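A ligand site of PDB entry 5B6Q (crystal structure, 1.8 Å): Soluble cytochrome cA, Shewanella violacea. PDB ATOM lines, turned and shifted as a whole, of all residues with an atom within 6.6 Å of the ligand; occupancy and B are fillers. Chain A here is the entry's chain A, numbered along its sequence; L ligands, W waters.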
ATOM      1  N   VAL A   6      27.456   3.010 -18.085  1.00  0.00           N
ATOM      2  CA  VAL A   6      26.354   2.094 -17.815  1.00  0.00           C
ATOM      3  C   VAL A   6      26.793   0.661 -18.039  1.00  0.00           C
ATOM      4  O   VAL A   6      26.526  -0.218 -17.201  1.00  0.00           O
ATOM      5  CB  VAL A   6      25.122   2.393 -18.706  1.00  0.00           C
ATOM      6  CG1 VAL A   6      24.037   1.345 -18.474  1.00  0.00           C
ATOM      7  CG2 VAL A   6      24.585   3.783 -18.402  1.00  0.00           C
ATOM      8  N   TYR A   7      27.483   0.427 -19.149  1.00  0.00           N
ATOM      9  CA  TYR A   7      28.010  -0.881 -19.478  1.00  0.00           C
ATOM     10  C   TYR A   7      28.935  -1.414 -18.386  1.00  0.00           C
ATOM     11  O   TYR A   7      28.831  -2.573 -17.981  1.00  0.00           O
ATOM     12  CB  TYR A   7      28.758  -0.852 -20.816  1.00  0.00           C
ATOM     13  CG  TYR A   7      29.417  -2.161 -21.179  1.00  0.00           C
ATOM     14  CD1 TYR A   7      28.705  -3.188 -21.791  1.00  0.00           C
ATOM     15  CD2 TYR A   7      30.767  -2.389 -20.886  1.00  0.00           C
ATOM     16  CE1 TYR A   7      29.302  -4.386 -22.112  1.00  0.00           C
ATOM     17  CE2 TYR A   7      31.373  -3.589 -21.204  1.00  0.00           C
ATOM     18  CZ  TYR A   7      30.634  -4.591 -21.815  1.00  0.00           C
ATOM     19  OH  TYR A   7      31.231  -5.789 -22.135  1.00  0.00           O
ATOM     20  N   ALA A  10      26.908  -2.360 -15.186  1.00  0.00           N
ATOM     21  CA  ALA A  10      25.725  -3.206 -15.325  1.00  0.00           C
ATOM     22  C   ALA A  10      25.770  -4.195 -16.483  1.00  0.00           C
ATOM     23  O   ALA A  10      25.890  -5.408 -16.281  1.00  0.00           O
ATOM     24  CB  ALA A  10      24.474  -2.332 -15.449  1.00  0.00           C
ATOM     25  N   CYS A  11      25.662  -3.685 -17.708  1.00  0.00           N
ATOM     26  CA  CYS A  11      25.477  -4.533 -18.890  1.00  0.00           C
ATOM     27  C   CYS A  11      26.600  -5.561 -19.099  1.00  0.00           C
ATOM     28  O   CYS A  11      26.353  -6.681 -19.539  1.00  0.00           O
ATOM     29  CB  CYS A  11      25.345  -3.673 -20.137  1.00  0.00           C
ATOM     30  SG  CYS A  11      24.247  -2.292 -19.895  1.00  0.00           S
ATOM     31  N   HIS A  12      27.824  -5.166 -18.766  1.00  0.00           N
ATOM     32  CA  HIS A  12      28.997  -6.007 -19.001  1.00  0.00           C
ATOM     33  C   HIS A  12      28.862  -7.390 -18.362  1.00  0.00           C
ATOM     34  O   HIS A  12      29.433  -8.363 -18.850  1.00  0.00           O
ATOM     35  CB  HIS A  12      30.254  -5.337 -18.459  1.00  0.00           C
ATOM     36  CG  HIS A  12      30.411  -5.477 -16.979  1.00  0.00           C
ATOM     37  ND1 HIS A  12      31.137  -6.505 -16.408  1.00  0.00           N
ATOM     38  CD2 HIS A  12      29.897  -4.769 -15.948  1.00  0.00           C
ATOM     39  CE1 HIS A  12      31.085  -6.402 -15.094  1.00  0.00           C
ATOM     40  NE2 HIS A  12      30.338  -5.357 -14.785  1.00  0.00           N
ATOM     41  N   ILE A  13      28.125  -7.471 -17.253  1.00  0.00           N
ATOM     42  CA  ILE A  13      28.008  -8.704 -16.481  1.00  0.00           C
ATOM     43  C   ILE A  13      27.652  -9.898 -17.373  1.00  0.00           C
ATOM     44  O   ILE A  13      28.252 -10.968 -17.244  1.00  0.00           O
ATOM     45  CB  ILE A  13      26.955  -8.565 -15.365  1.00  0.00           C
ATOM     46  CG1 ILE A  13      27.441  -7.556 -14.326  1.00  0.00           C
ATOM     47  CG2 ILE A  13      26.666  -9.915 -14.711  1.00  0.00           C
ATOM     48  CD1 ILE A  13      26.339  -7.043 -13.427  1.00  0.00           C
ATOM     49  N   CYS A  14      26.723  -9.693 -18.296  1.00  0.00           N
ATOM     50  CA  CYS A  14      26.272 -10.764 -19.174  1.00  0.00           C
ATOM     51  C   CYS A  14      26.711 -10.571 -20.621  1.00  0.00           C
ATOM     52  O   CYS A  14      26.850 -11.540 -21.358  1.00  0.00           O
ATOM     53  CB  CYS A  14      24.744 -10.897 -19.108  1.00  0.00           C
ATOM     54  SG  CYS A  14      24.073 -11.058 -17.439  1.00  0.00           S
ATOM     55  N   HIS A  15      26.933  -9.318 -21.014  1.00  0.00           N
ATOM     56  CA  HIS A  15      27.232  -9.023 -22.413  1.00  0.00           C
ATOM     57  C   HIS A  15      28.720  -9.017 -22.764  1.00  0.00           C
ATOM     58  O   HIS A  15      29.071  -9.076 -23.938  1.00  0.00           O
ATOM     59  CB  HIS A  15      26.629  -7.671 -22.805  1.00  0.00           C
ATOM     60  CG  HIS A  15      25.148  -7.710 -23.011  1.00  0.00           C
ATOM     61  ND1 HIS A  15      24.574  -8.038 -24.220  1.00  0.00           N
ATOM     62  CD2 HIS A  15      24.126  -7.446 -22.157  1.00  0.00           C
ATOM     63  CE1 HIS A  15      23.256  -7.979 -24.106  1.00  0.00           C
ATOM     64  NE2 HIS A  15      22.965  -7.617 -22.862  1.00  0.00           N
ATOM     65  N   VAL A  19      26.820 -14.168 -22.297  1.00  0.00           N
ATOM     66  CA  VAL A  19      26.323 -15.299 -21.518  1.00  0.00           C
ATOM     67  C   VAL A  19      24.857 -15.551 -21.864  1.00  0.00           C
ATOM     68  O   VAL A  19      24.108 -14.616 -22.135  1.00  0.00           O
ATOM     69  CB  VAL A  19      26.511 -15.058 -20.005  1.00  0.00           C
ATOM     70  CG1 VAL A  19      26.108 -16.285 -19.211  1.00  0.00           C
ATOM     71  CG2 VAL A  19      27.955 -14.693 -19.701  1.00  0.00           C
ATOM     72  N   ALA A  20      24.480 -16.829 -21.861  1.00  0.00           N
ATOM     73  CA  ALA A  20      23.110 -17.279 -22.147  1.00  0.00           C
ATOM     74  C   ALA A  20      22.564 -16.683 -23.436  1.00  0.00           C
ATOM     75  O   ALA A  20      21.381 -16.368 -23.525  1.00  0.00           O
ATOM     76  CB  ALA A  20      22.196 -16.950 -20.987  1.00  0.00           C
ATOM     77  N   GLY A  21      23.436 -16.514 -24.428  1.00  0.00           N
ATOM     78  CA  GLY A  21      23.021 -16.006 -25.722  1.00  0.00           C
ATOM     79  C   GLY A  21      22.935 -14.494 -25.839  1.00  0.00           C
ATOM     80  O   GLY A  21      22.480 -13.980 -26.860  1.00  0.00           O
ATOM     81  N   ALA A  22      23.371 -13.777 -24.809  1.00  0.00           N
ATOM     82  CA  ALA A  22      23.392 -12.313 -24.887  1.00  0.00           C
ATOM     83  C   ALA A  22      24.294 -11.893 -26.041  1.00  0.00           C
ATOM     84  O   ALA A  22      25.361 -12.480 -26.251  1.00  0.00           O
ATOM     85  CB  ALA A  22      23.876 -11.708 -23.563  1.00  0.00           C
ATOM     86  N   PRO A  23      23.852 -10.908 -26.837  1.00  0.00           N
ATOM     87  CA  PRO A  23      24.734 -10.423 -27.902  1.00  0.00           C
ATOM     88  C   PRO A  23      25.991  -9.805 -27.308  1.00  0.00           C
ATOM     89  O   PRO A  23      25.907  -8.861 -26.514  1.00  0.00           O
ATOM     90  CB  PRO A  23      23.871  -9.374 -28.627  1.00  0.00           C
ATOM     91  CG  PRO A  23      22.760  -9.055 -27.663  1.00  0.00           C
ATOM     92  CD  PRO A  23      22.517 -10.302 -26.898  1.00  0.00           C
ATOM     93  N   TRP A  31      25.050  -7.696 -33.055  1.00  0.00           N
ATOM     94  CA  TRP A  31      24.137  -6.625 -32.682  1.00  0.00           C
ATOM     95  C   TRP A  31      23.343  -6.061 -33.867  1.00  0.00           C
ATOM     96  O   TRP A  31      22.277  -5.488 -33.671  1.00  0.00           O
ATOM     97  CB  TRP A  31      24.904  -5.487 -31.994  1.00  0.00           C
ATOM     98  CG  TRP A  31      25.147  -5.756 -30.537  1.00  0.00           C
ATOM     99  CD1 TRP A  31      26.279  -6.272 -29.972  1.00  0.00           C
ATOM    100  CD2 TRP A  31      24.235  -5.519 -29.455  1.00  0.00           C
ATOM    101  NE1 TRP A  31      26.127  -6.369 -28.606  1.00  0.00           N
ATOM    102  CE2 TRP A  31      24.880  -5.913 -28.262  1.00  0.00           C
ATOM    103  CE3 TRP A  31      22.925  -5.014 -29.386  1.00  0.00           C
ATOM    104  CZ2 TRP A  31      24.270  -5.812 -27.016  1.00  0.00           C
ATOM    105  CZ3 TRP A  31      22.325  -4.922 -28.146  1.00  0.00           C
ATOM    106  CH2 TRP A  31      22.986  -5.319 -26.977  1.00  0.00           C
ATOM    107  N   ARG A  34      19.702  -6.853 -34.102  1.00  0.00           N
ATOM    108  CA  ARG A  34      18.988  -6.307 -32.962  1.00  0.00           C
ATOM    109  C   ARG A  34      18.839  -4.798 -33.079  1.00  0.00           C
ATOM    110  O   ARG A  34      17.750  -4.265 -32.859  1.00  0.00           O
ATOM    111  CB  ARG A  34      19.704  -6.709 -31.673  1.00  0.00           C
ATOM    112  CG  ARG A  34      19.705  -8.230 -31.510  1.00  0.00           C
ATOM    113  CD  ARG A  34      20.499  -8.671 -30.319  1.00  0.00           C
ATOM    114  NE  ARG A  34      20.196 -10.053 -29.943  1.00  0.00           N
ATOM    115  CZ  ARG A  34      20.895 -11.116 -30.336  1.00  0.00           C
ATOM    116  NH1 ARG A  34      21.939 -10.962 -31.136  1.00  0.00           N
ATOM    117  NH2 ARG A  34      20.541 -12.324 -29.922  1.00  0.00           N
ATOM    118  N   GLN A  37      15.960  -3.511 -35.279  1.00  0.00           N
ATOM    119  CA  GLN A  37      14.647  -3.496 -34.715  1.00  0.00           C
ATOM    120  C   GLN A  37      14.234  -2.072 -34.340  1.00  0.00           C
ATOM    121  O   GLN A  37      13.092  -1.801 -34.188  1.00  0.00           O
ATOM    122  CB  GLN A  37      14.511  -4.438 -33.499  1.00  0.00           C
ATOM    123  CG  GLN A  37      14.902  -5.863 -33.691  1.00  0.00           C
ATOM    124  CD  GLN A  37      14.539  -6.752 -32.484  1.00  0.00           C
ATOM    125  OE1 GLN A  37      13.388  -6.816 -32.100  1.00  0.00           O
ATOM    126  NE2 GLN A  37      15.503  -7.447 -31.919  1.00  0.00           N
ATOM    127  N   THR A  41      12.466   0.273 -29.718  1.00  0.00           N
ATOM    128  CA  THR A  41      12.057  -1.095 -29.417  1.00  0.00           C
ATOM    129  C   THR A  41      13.027  -1.761 -28.445  1.00  0.00           C
ATOM    130  O   THR A  41      12.604  -2.430 -27.485  1.00  0.00           O
ATOM    131  CB  THR A  41      11.967  -1.942 -30.693  1.00  0.00           C
ATOM    132  OG1 THR A  41      10.914  -1.446 -31.531  1.00  0.00           O
ATOM    133  CG2 THR A  41      11.699  -3.408 -30.360  1.00  0.00           C
ATOM    134  N   LEU A  42      14.321  -1.568 -28.667  1.00  0.00           N
ATOM    135  CA  LEU A  42      15.341  -2.167 -27.815  1.00  0.00           C
ATOM    136  C   LEU A  42      15.293  -1.616 -26.394  1.00  0.00           C
ATOM    137  O   LEU A  42      15.403  -2.378 -25.428  1.00  0.00           O
ATOM    138  CB  LEU A  42      16.736  -1.944 -28.413  1.00  0.00           C
ATOM    139  CG  LEU A  42      16.995  -2.693 -29.727  1.00  0.00           C
ATOM    140  CD1 LEU A  42      18.445  -2.520 -30.146  1.00  0.00           C
ATOM    141  CD2 LEU A  42      16.610  -4.159 -29.609  1.00  0.00           C
ATOM    142  N   VAL A  43      15.133  -0.308 -26.258  1.00  0.00           N
ATOM    143  CA  VAL A  43      15.050   0.288 -24.925  1.00  0.00           C
ATOM    144  C   VAL A  43      13.835  -0.266 -24.189  1.00  0.00           C
ATOM    145  O   VAL A  43      13.928  -0.629 -23.013  1.00  0.00           O
ATOM    146  CB  VAL A  43      14.969   1.833 -24.990  1.00  0.00           C
ATOM    147  CG1 VAL A  43      14.672   2.422 -23.633  1.00  0.00           C
ATOM    148  CG2 VAL A  43      16.270   2.401 -25.539  1.00  0.00           C
ATOM    149  N   THR A  45      12.386  -3.159 -24.644  1.00  0.00           N
ATOM    150  CA  THR A  45      12.694  -4.552 -24.311  1.00  0.00           C
ATOM    151  C   THR A  45      13.597  -4.669 -23.068  1.00  0.00           C
ATOM    152  O   THR A  45      13.351  -5.509 -22.197  1.00  0.00           O
ATOM    153  CB  THR A  45      13.357  -5.267 -25.497  1.00  0.00           C
ATOM    154  OG1 THR A  45      12.384  -5.438 -26.528  1.00  0.00           O
ATOM    155  CG2 THR A  45      13.913  -6.619 -25.078  1.00  0.00           C
ATOM    156  N   VAL A  46      14.612  -3.821 -22.966  1.00  0.00           N
ATOM    157  CA  VAL A  46      15.530  -3.867 -21.822  1.00  0.00           C
ATOM    158  C   VAL A  46      14.808  -3.568 -20.523  1.00  0.00           C
ATOM    159  O   VAL A  46      15.051  -4.204 -19.492  1.00  0.00           O
ATOM    160  CB  VAL A  46      16.687  -2.862 -21.993  1.00  0.00           C
ATOM    161  CG1 VAL A  46      17.546  -2.814 -20.747  1.00  0.00           C
ATOM    162  CG2 VAL A  46      17.528  -3.241 -23.192  1.00  0.00           C
ATOM    163  N   LYS A  50      13.819  -9.636 -21.214  1.00  0.00           N
ATOM    164  CA  LYS A  50      13.610 -10.569 -22.314  1.00  0.00           C
ATOM    165  C   LYS A  50      14.313 -11.878 -22.000  1.00  0.00           C
ATOM    166  O   LYS A  50      15.551 -11.942 -22.001  1.00  0.00           O
ATOM    167  CB  LYS A  50      14.122  -9.976 -23.630  1.00  0.00           C
ATOM    168  CG  LYS A  50      14.006 -10.922 -24.825  1.00  0.00           C
ATOM    169  CD  LYS A  50      14.200 -10.195 -26.149  1.00  0.00           C
ATOM    170  CE  LYS A  50      14.075 -11.161 -27.324  1.00  0.00           C
ATOM    171  NZ  LYS A  50      13.884 -10.462 -28.626  1.00  0.00           N
ATOM    172  N   GLY A  51      13.521 -12.913 -21.724  1.00  0.00           N
ATOM    173  CA  GLY A  51      14.049 -14.215 -21.370  1.00  0.00           C
ATOM    174  C   GLY A  51      14.992 -14.187 -20.184  1.00  0.00           C
ATOM    175  O   GLY A  51      14.592 -13.875 -19.052  1.00  0.00           O
ATOM    176  N   ALA A  52      16.259 -14.491 -20.453  1.00  0.00           N
ATOM    177  CA  ALA A  52      17.279 -14.557 -19.408  1.00  0.00           C
ATOM    178  C   ALA A  52      17.683 -13.172 -18.898  1.00  0.00           C
ATOM    179  O   ALA A  52      18.209 -13.062 -17.786  1.00  0.00           O
ATOM    180  CB  ALA A  52      18.499 -15.305 -19.916  1.00  0.00           C
ATOM    181  N   MET A  53      17.456 -12.131 -19.682  1.00  0.00           N
ATOM    182  CA  MET A  53      17.767 -10.786 -19.207  1.00  0.00           C
ATOM    183  C   MET A  53      16.648 -10.262 -18.319  1.00  0.00           C
ATOM    184  O   MET A  53      15.481 -10.242 -18.708  1.00  0.00           O
ATOM    185  CB  MET A  53      17.999  -9.812 -20.365  1.00  0.00           C
ATOM    186  CG  MET A  53      18.438  -8.432 -19.875  1.00  0.00           C
ATOM    187  SD  MET A  53      18.835  -7.301 -21.221  1.00  0.00           S
ATOM    188  CE  MET A  53      17.244  -7.215 -22.033  1.00  0.00           C
ATOM    189  N   PRO A  54      17.009  -9.840 -17.101  1.00  0.00           N
ATOM    190  CA  PRO A  54      16.064  -9.255 -16.153  1.00  0.00           C
ATOM    191  C   PRO A  54      15.687  -7.814 -16.509  1.00  0.00           C
ATOM    192  O   PRO A  54      16.517  -7.093 -17.065  1.00  0.00           O
ATOM    193  CB  PRO A  54      16.827  -9.301 -14.833  1.00  0.00           C
ATOM    194  CG  PRO A  54      18.262  -9.198 -15.240  1.00  0.00           C
ATOM    195  CD  PRO A  54      18.359  -9.955 -16.540  1.00  0.00           C
ATOM    196  N   GLY A  56      15.427  -4.112 -16.825  1.00  0.00           N
ATOM    197  CA  GLY A  56      16.314  -3.051 -16.406  1.00  0.00           C
ATOM    198  C   GLY A  56      17.784  -3.303 -16.701  1.00  0.00           C
ATOM    199  O   GLY A  56      18.611  -2.378 -16.628  1.00  0.00           O
ATOM    200  N   GLY A  57      18.123  -4.550 -17.029  1.00  0.00           N
ATOM    201  CA  GLY A  57      19.493  -4.935 -17.310  1.00  0.00           C
ATOM    202  C   GLY A  57      20.437  -4.605 -16.169  1.00  0.00           C
ATOM    203  O   GLY A  57      21.595  -4.238 -16.387  1.00  0.00           O
ATOM    204  N   MET A  58      19.928  -4.722 -14.943  1.00  0.00           N
ATOM    205  CA  MET A  58      20.674  -4.453 -13.709  1.00  0.00           C
ATOM    206  C   MET A  58      21.265  -3.044 -13.592  1.00  0.00           C
ATOM    207  O   MET A  58      22.218  -2.824 -12.847  1.00  0.00           O
ATOM    208  CB  MET A  58      21.794  -5.477 -13.542  1.00  0.00           C
ATOM    209  CG  MET A  58      21.276  -6.881 -13.338  1.00  0.00           C
ATOM    210  SD  MET A  58      22.630  -8.001 -13.038  1.00  0.00           S
ATOM    211  CE  MET A  58      23.139  -7.489 -11.395  1.00  0.00           C
ATOM    212  N   CYS A  59      20.709  -2.112 -14.341  1.00  0.00           N
ATOM    213  CA  CYS A  59      20.981  -0.709 -14.107  1.00  0.00           C
ATOM    214  C   CYS A  59      19.841  -0.137 -13.268  1.00  0.00           C
ATOM    215  O   CYS A  59      18.680  -0.240 -13.647  1.00  0.00           O
ATOM    216  CB  CYS A  59      21.129   0.062 -15.420  1.00  0.00           C
ATOM    217  SG  CYS A  59      21.363   1.815 -15.154  1.00  0.00           S
ATOM    218  N   CYS A  62      18.845   4.058 -14.668  1.00  0.00           N
ATOM    219  CA  CYS A  62      18.966   4.371 -16.093  1.00  0.00           C
ATOM    220  C   CYS A  62      17.735   5.027 -16.704  1.00  0.00           C
ATOM    221  O   CYS A  62      16.627   4.506 -16.640  1.00  0.00           O
ATOM    222  CB  CYS A  62      19.290   3.091 -16.881  1.00  0.00           C
ATOM    223  SG  CYS A  62      21.046   2.668 -16.965  1.00  0.00           S
ATOM    224  N   ASP A  66      20.076   6.764 -21.202  1.00  0.00           N
ATOM    225  CA  ASP A  66      21.130   5.925 -20.645  1.00  0.00           C
ATOM    226  C   ASP A  66      21.130   4.554 -21.317  1.00  0.00           C
ATOM    227  O   ASP A  66      22.181   4.077 -21.735  1.00  0.00           O
ATOM    228  CB  ASP A  66      20.975   5.759 -19.141  1.00  0.00           C
ATOM    229  CG  ASP A  66      21.170   7.051 -18.381  1.00  0.00           C
ATOM    230  OD1 ASP A  66      21.798   7.987 -18.933  1.00  0.00           O
ATOM    231  OD2 ASP A  66      20.703   7.130 -17.233  1.00  0.00           O
ATOM    232  N   TYR A  67      19.959   3.948 -21.412  1.00  0.00           N
ATOM    233  CA  TYR A  67      19.807   2.638 -22.054  1.00  0.00           C
ATOM    234  C   TYR A  67      20.248   2.667 -23.506  1.00  0.00           C
ATOM    235  O   TYR A  67      20.966   1.789 -23.968  1.00  0.00           O
ATOM    236  CB  TYR A  67      18.365   2.152 -21.958  1.00  0.00           C
ATOM    237  CG  TYR A  67      17.994   1.577 -20.610  1.00  0.00           C
ATOM    238  CD1 TYR A  67      18.808   0.633 -19.991  1.00  0.00           C
ATOM    239  CD2 TYR A  67      16.846   1.991 -19.952  1.00  0.00           C
ATOM    240  CE1 TYR A  67      18.475   0.112 -18.765  1.00  0.00           C
ATOM    241  CE2 TYR A  67      16.514   1.477 -18.719  1.00  0.00           C
ATOM    242  CZ  TYR A  67      17.323   0.542 -18.123  1.00  0.00           C
ATOM    243  OH  TYR A  67      16.981   0.030 -16.892  1.00  0.00           O
ATOM    244  N   LYS A  68      19.804   3.693 -24.216  1.00  0.00           N
ATOM    245  CA  LYS A  68      20.177   3.875 -25.612  1.00  0.00           C
ATOM    246  C   LYS A  68      21.700   4.047 -25.760  1.00  0.00           C
ATOM    247  O   LYS A  68      22.307   3.425 -26.633  1.00  0.00           O
ATOM    248  CB  LYS A  68      19.432   5.078 -26.188  1.00  0.00           C
ATOM    249  CG  LYS A  68      19.802   5.469 -27.593  1.00  0.00           C
ATOM    250  CD  LYS A  68      18.972   6.681 -28.015  1.00  0.00           C
ATOM    251  CE  LYS A  68      19.459   7.257 -29.329  1.00  0.00           C
ATOM    252  NZ  LYS A  68      18.664   8.463 -29.728  1.00  0.00           N
ATOM    253  N   ALA A  70      24.031   2.976 -23.772  1.00  0.00           N
ATOM    254  CA  ALA A  70      24.652   1.709 -23.434  1.00  0.00           C
ATOM    255  C   ALA A  70      24.623   0.740 -24.616  1.00  0.00           C
ATOM    256  O   ALA A  70      25.614   0.083 -24.916  1.00  0.00           O
ATOM    257  CB  ALA A  70      23.971   1.084 -22.221  1.00  0.00           C
ATOM    258  N   ILE A  71      23.466   0.667 -25.263  1.00  0.00           N
ATOM    259  CA  ILE A  71      23.290  -0.183 -26.443  1.00  0.00           C
ATOM    260  C   ILE A  71      24.232   0.258 -27.573  1.00  0.00           C
ATOM    261  O   ILE A  71      24.903  -0.570 -28.199  1.00  0.00           O
ATOM    262  CB  ILE A  71      21.824  -0.158 -26.936  1.00  0.00           C
ATOM    263  CG1 ILE A  71      20.908  -0.788 -25.885  1.00  0.00           C
ATOM    264  CG2 ILE A  71      21.678  -0.908 -28.255  1.00  0.00           C
ATOM    265  CD1 ILE A  71      19.422  -0.735 -26.223  1.00  0.00           C
ATOM    266  N   MET A  74      27.673  -0.955 -26.907  1.00  0.00           N
ATOM    267  CA  MET A  74      27.859  -2.396 -27.079  1.00  0.00           C
ATOM    268  C   MET A  74      27.825  -2.780 -28.557  1.00  0.00           C
ATOM    269  O   MET A  74      28.460  -3.759 -28.964  1.00  0.00           O
ATOM    270  CB  MET A  74      26.792  -3.184 -26.316  1.00  0.00           C
ATOM    271  CG  MET A  74      26.958  -3.118 -24.799  1.00  0.00           C
ATOM    272  SD  MET A  74      25.997  -4.339 -23.885  1.00  0.00           S
ATOM    273  CE  MET A  74      24.334  -3.700 -24.079  1.00  0.00           C
HETATM  274 FE1  LIG L   1      20.955  -7.604 -22.079  1.00  0.00          FE
HETATM  275  C1  LIG L   1      19.811  -9.072 -24.932  1.00  0.00           C
HETATM  276  C2  LIG L   1      20.691  -4.476 -23.698  1.00  0.00           C
HETATM  277  C3  LIG L   1      22.254  -5.958 -19.308  1.00  0.00           C
HETATM  278  C4  LIG L   1      21.393 -10.564 -20.589  1.00  0.00           C
HETATM  279  N1  LIG L   1      20.441  -6.917 -23.890  1.00  0.00           N
HETATM  280  C5  LIG L   1      19.902  -7.711 -24.892  1.00  0.00           C
HETATM  281  C6  LIG L   1      19.419  -6.925 -25.943  1.00  0.00           C
HETATM  282  C7  LIG L   1      19.650  -5.633 -25.616  1.00  0.00           C
HETATM  283  C8  LIG L   1      20.293  -5.620 -24.361  1.00  0.00           C
HETATM  284  C9  LIG L   1      19.279  -4.443 -26.470  1.00  0.00           C
HETATM  285  C10 LIG L   1      18.752  -7.422 -27.200  1.00  0.00           C
HETATM  286  C11 LIG L   1      17.250  -7.636 -26.996  1.00  0.00           C
HETATM  287  C12 LIG L   1      16.602  -8.078 -28.293  1.00  0.00           C
HETATM  288  O1  LIG L   1      15.529  -7.571 -28.664  1.00  0.00           O
HETATM  289  O2  LIG L   1      17.140  -8.967 -28.977  1.00  0.00           O
HETATM  290  N2  LIG L   1      21.416  -5.587 -21.640  1.00  0.00           N
HETATM  291  C13 LIG L   1      21.213  -4.507 -22.404  1.00  0.00           C
HETATM  292  C14 LIG L   1      21.632  -3.331 -21.715  1.00  0.00           C
HETATM  293  C15 LIG L   1      22.071  -3.713 -20.474  1.00  0.00           C
HETATM  294  C16 LIG L   1      21.911  -5.194 -20.442  1.00  0.00           C
HETATM  295  C17 LIG L   1      21.595  -1.921 -22.262  1.00  0.00           C
HETATM  296  C18 LIG L   1      22.622  -2.838 -19.412  1.00  0.00           C
HETATM  297  C19 LIG L   1      21.909  -1.819 -18.907  1.00  0.00           C
HETATM  298  N3  LIG L   1      21.738  -8.158 -20.244  1.00  0.00           N
HETATM  299  C20 LIG L   1      22.140  -7.349 -19.223  1.00  0.00           C
HETATM  300  C21 LIG L   1      22.425  -8.166 -18.108  1.00  0.00           C
HETATM  301  C22 LIG L   1      22.170  -9.481 -18.484  1.00  0.00           C
HETATM  302  C23 LIG L   1      21.731  -9.462 -19.831  1.00  0.00           C
HETATM  303  C24 LIG L   1      22.908  -7.662 -16.769  1.00  0.00           C
HETATM  304  C25 LIG L   1      22.343 -10.694 -17.646  1.00  0.00           C
HETATM  305  C26 LIG L   1      21.776 -10.815 -16.447  1.00  0.00           C
HETATM  306  N4  LIG L   1      20.689  -9.369 -22.672  1.00  0.00           N
HETATM  307  C27 LIG L   1      20.909 -10.466 -21.903  1.00  0.00           C
HETATM  308  C28 LIG L   1      20.561 -11.674 -22.656  1.00  0.00           C
HETATM  309  C29 LIG L   1      20.127 -11.265 -23.852  1.00  0.00           C
HETATM  310  C30 LIG L   1      20.190  -9.805 -23.841  1.00  0.00           C
HETATM  311  C31 LIG L   1      20.675 -13.102 -22.185  1.00  0.00           C
HETATM  312  C32 LIG L   1      19.636 -12.134 -24.988  1.00  0.00           C
HETATM  313  C33 LIG L   1      18.144 -12.353 -24.694  1.00  0.00           C
HETATM  314  C34 LIG L   1      17.468 -13.082 -25.822  1.00  0.00           C
HETATM  315  O3  LIG L   1      17.774 -12.831 -27.009  1.00  0.00           O
HETATM  316  O4  LIG L   1      16.597 -13.938 -25.557  1.00  0.00           O
HETATM  317  O   HOH W   1      15.823 -13.274 -29.073  1.00  0.00           O
HETATM  318  O   HOH W   2      16.841 -15.276 -23.259  1.00  0.00           O
HETATM  319  O   HOH W   3      13.705  -5.844 -28.800  1.00  0.00           O
HETATM  320  O   HOH W   4      14.285 -14.936 -26.069  1.00  0.00           O
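C25 of the ligand is bonded to SG of Cys 14, 1.8 Å away.
C18 of the ligand is covalently linked to SG of Cys 11 (1.8 Å).
FE1 of the ligand is bound by NE2 of His 15.
FE1 of the ligand is bound by SD of Met 53 (2.3 Å).
O1 of the ligand lies within hydrogen-bond range of NE2 of Gln 37.
An oxygen (O1) of the ligand is in salt-bridge range of the side-chain amino group (NZ) of Lys 50, 3.3 Å away.
The guanidinium group of Arg 34 lies within salt-bridge range of an oxygen (O2) of the ligand (3.4 Å).
O of Cys 14 is in hydrogen-bond range of N of Val 19.
ND1 of His 15 sits at hydrogen-bond distance from O of Pro 23.
OG1 of Thr 41 sits at hydrogen-bond distance from O of Gln 37.
The backbone carbonyl oxygen (O) of Val 46 sits at hydrogen-bond distance from the backbone NH (N) of Gly 56, at 2.7 Å.
The indole nitrogen (NE1) of Trp 31 is in hydrogen-bond range of the backbone carbonyl oxygen (O) of Pro 23 (3.3 Å).
OH of Tyr 67 lies within hydrogen-bond range of O of Gly 56.
The side-chain hydroxyl (OG1) of Thr 45 lies within hydrogen-bond range of the backbone carbonyl oxygen (O) of Thr 41 (3.2 Å).
The side-chain sulfur (SG) of Cys 62 is disulfide-bonded to the side-chain sulfur (SG) of Cys 59, at 2.0 Å.
CG1 of Val 6 touches C19 of the ligand, 3.8 Å away.
O of Ala 10 touches C24 of the ligand (3.8 Å).
O of Val 19 touches C31 of the ligand, at 3.8 Å.
O of Ala 20 touches C31 of the ligand (3.6 Å).
Gly 21 touches the ligand (O to C32, 3.9 Å).
CB of Ala 22 touches C28 of the ligand, 3.4 Å away.
Pro 23 touches the ligand (CD to C1, 3.6 Å).
Trp 31 touches the ligand.
Leu 42 touches the ligand.
Thr 45 touches the ligand.
Val 46 touches the ligand (CG2 to C2, 3.4 Å).
Ala 52 touches the ligand (CB to C31, 3.8 Å).
Pro 54 touches the ligand.
Gly 57 touches the ligand (O to C3, 3.5 Å).
Met 58 touches the ligand.
Tyr 67 touches the ligand.
Ala 70 touches the ligand.
Ile 71 touches the ligand.
Met 74 touches the ligand (CE to C14, 3.6 Å).
Within 4 Å of the ligand: Val 6, Ala 10, Cys 11, Cys 14, His 15, Val 19, Ala 20, Gly 21, Ala 22, Pro 23, Trp 31, Arg 34, Gln 37, Leu 42, Thr 45, Val 46, Lys 50, Ala 52, Met 53, Pro 54, Gly 57, Met 58, Tyr 67, Ala 70, Ile 71 and Met 74.
The nearest printed residue that does not touch the ligand is Cys 59 (4.04 Å).
Water W3 lies within hydrogen-bond range of O1 of the ligand (2.5 Å), OG1 of Thr 45 (2.7 Å) and OE1 of Gln 37 (3.5 Å).
Water W2 lies within hydrogen-bond range of O4 of the ligand (2.7 Å) and N of Ala 52 (3.0 Å).
Water W1 lies within hydrogen-bond range of an oxygen (O3) of the ligand and the side-chain amino group (NZ) of Lys 50.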
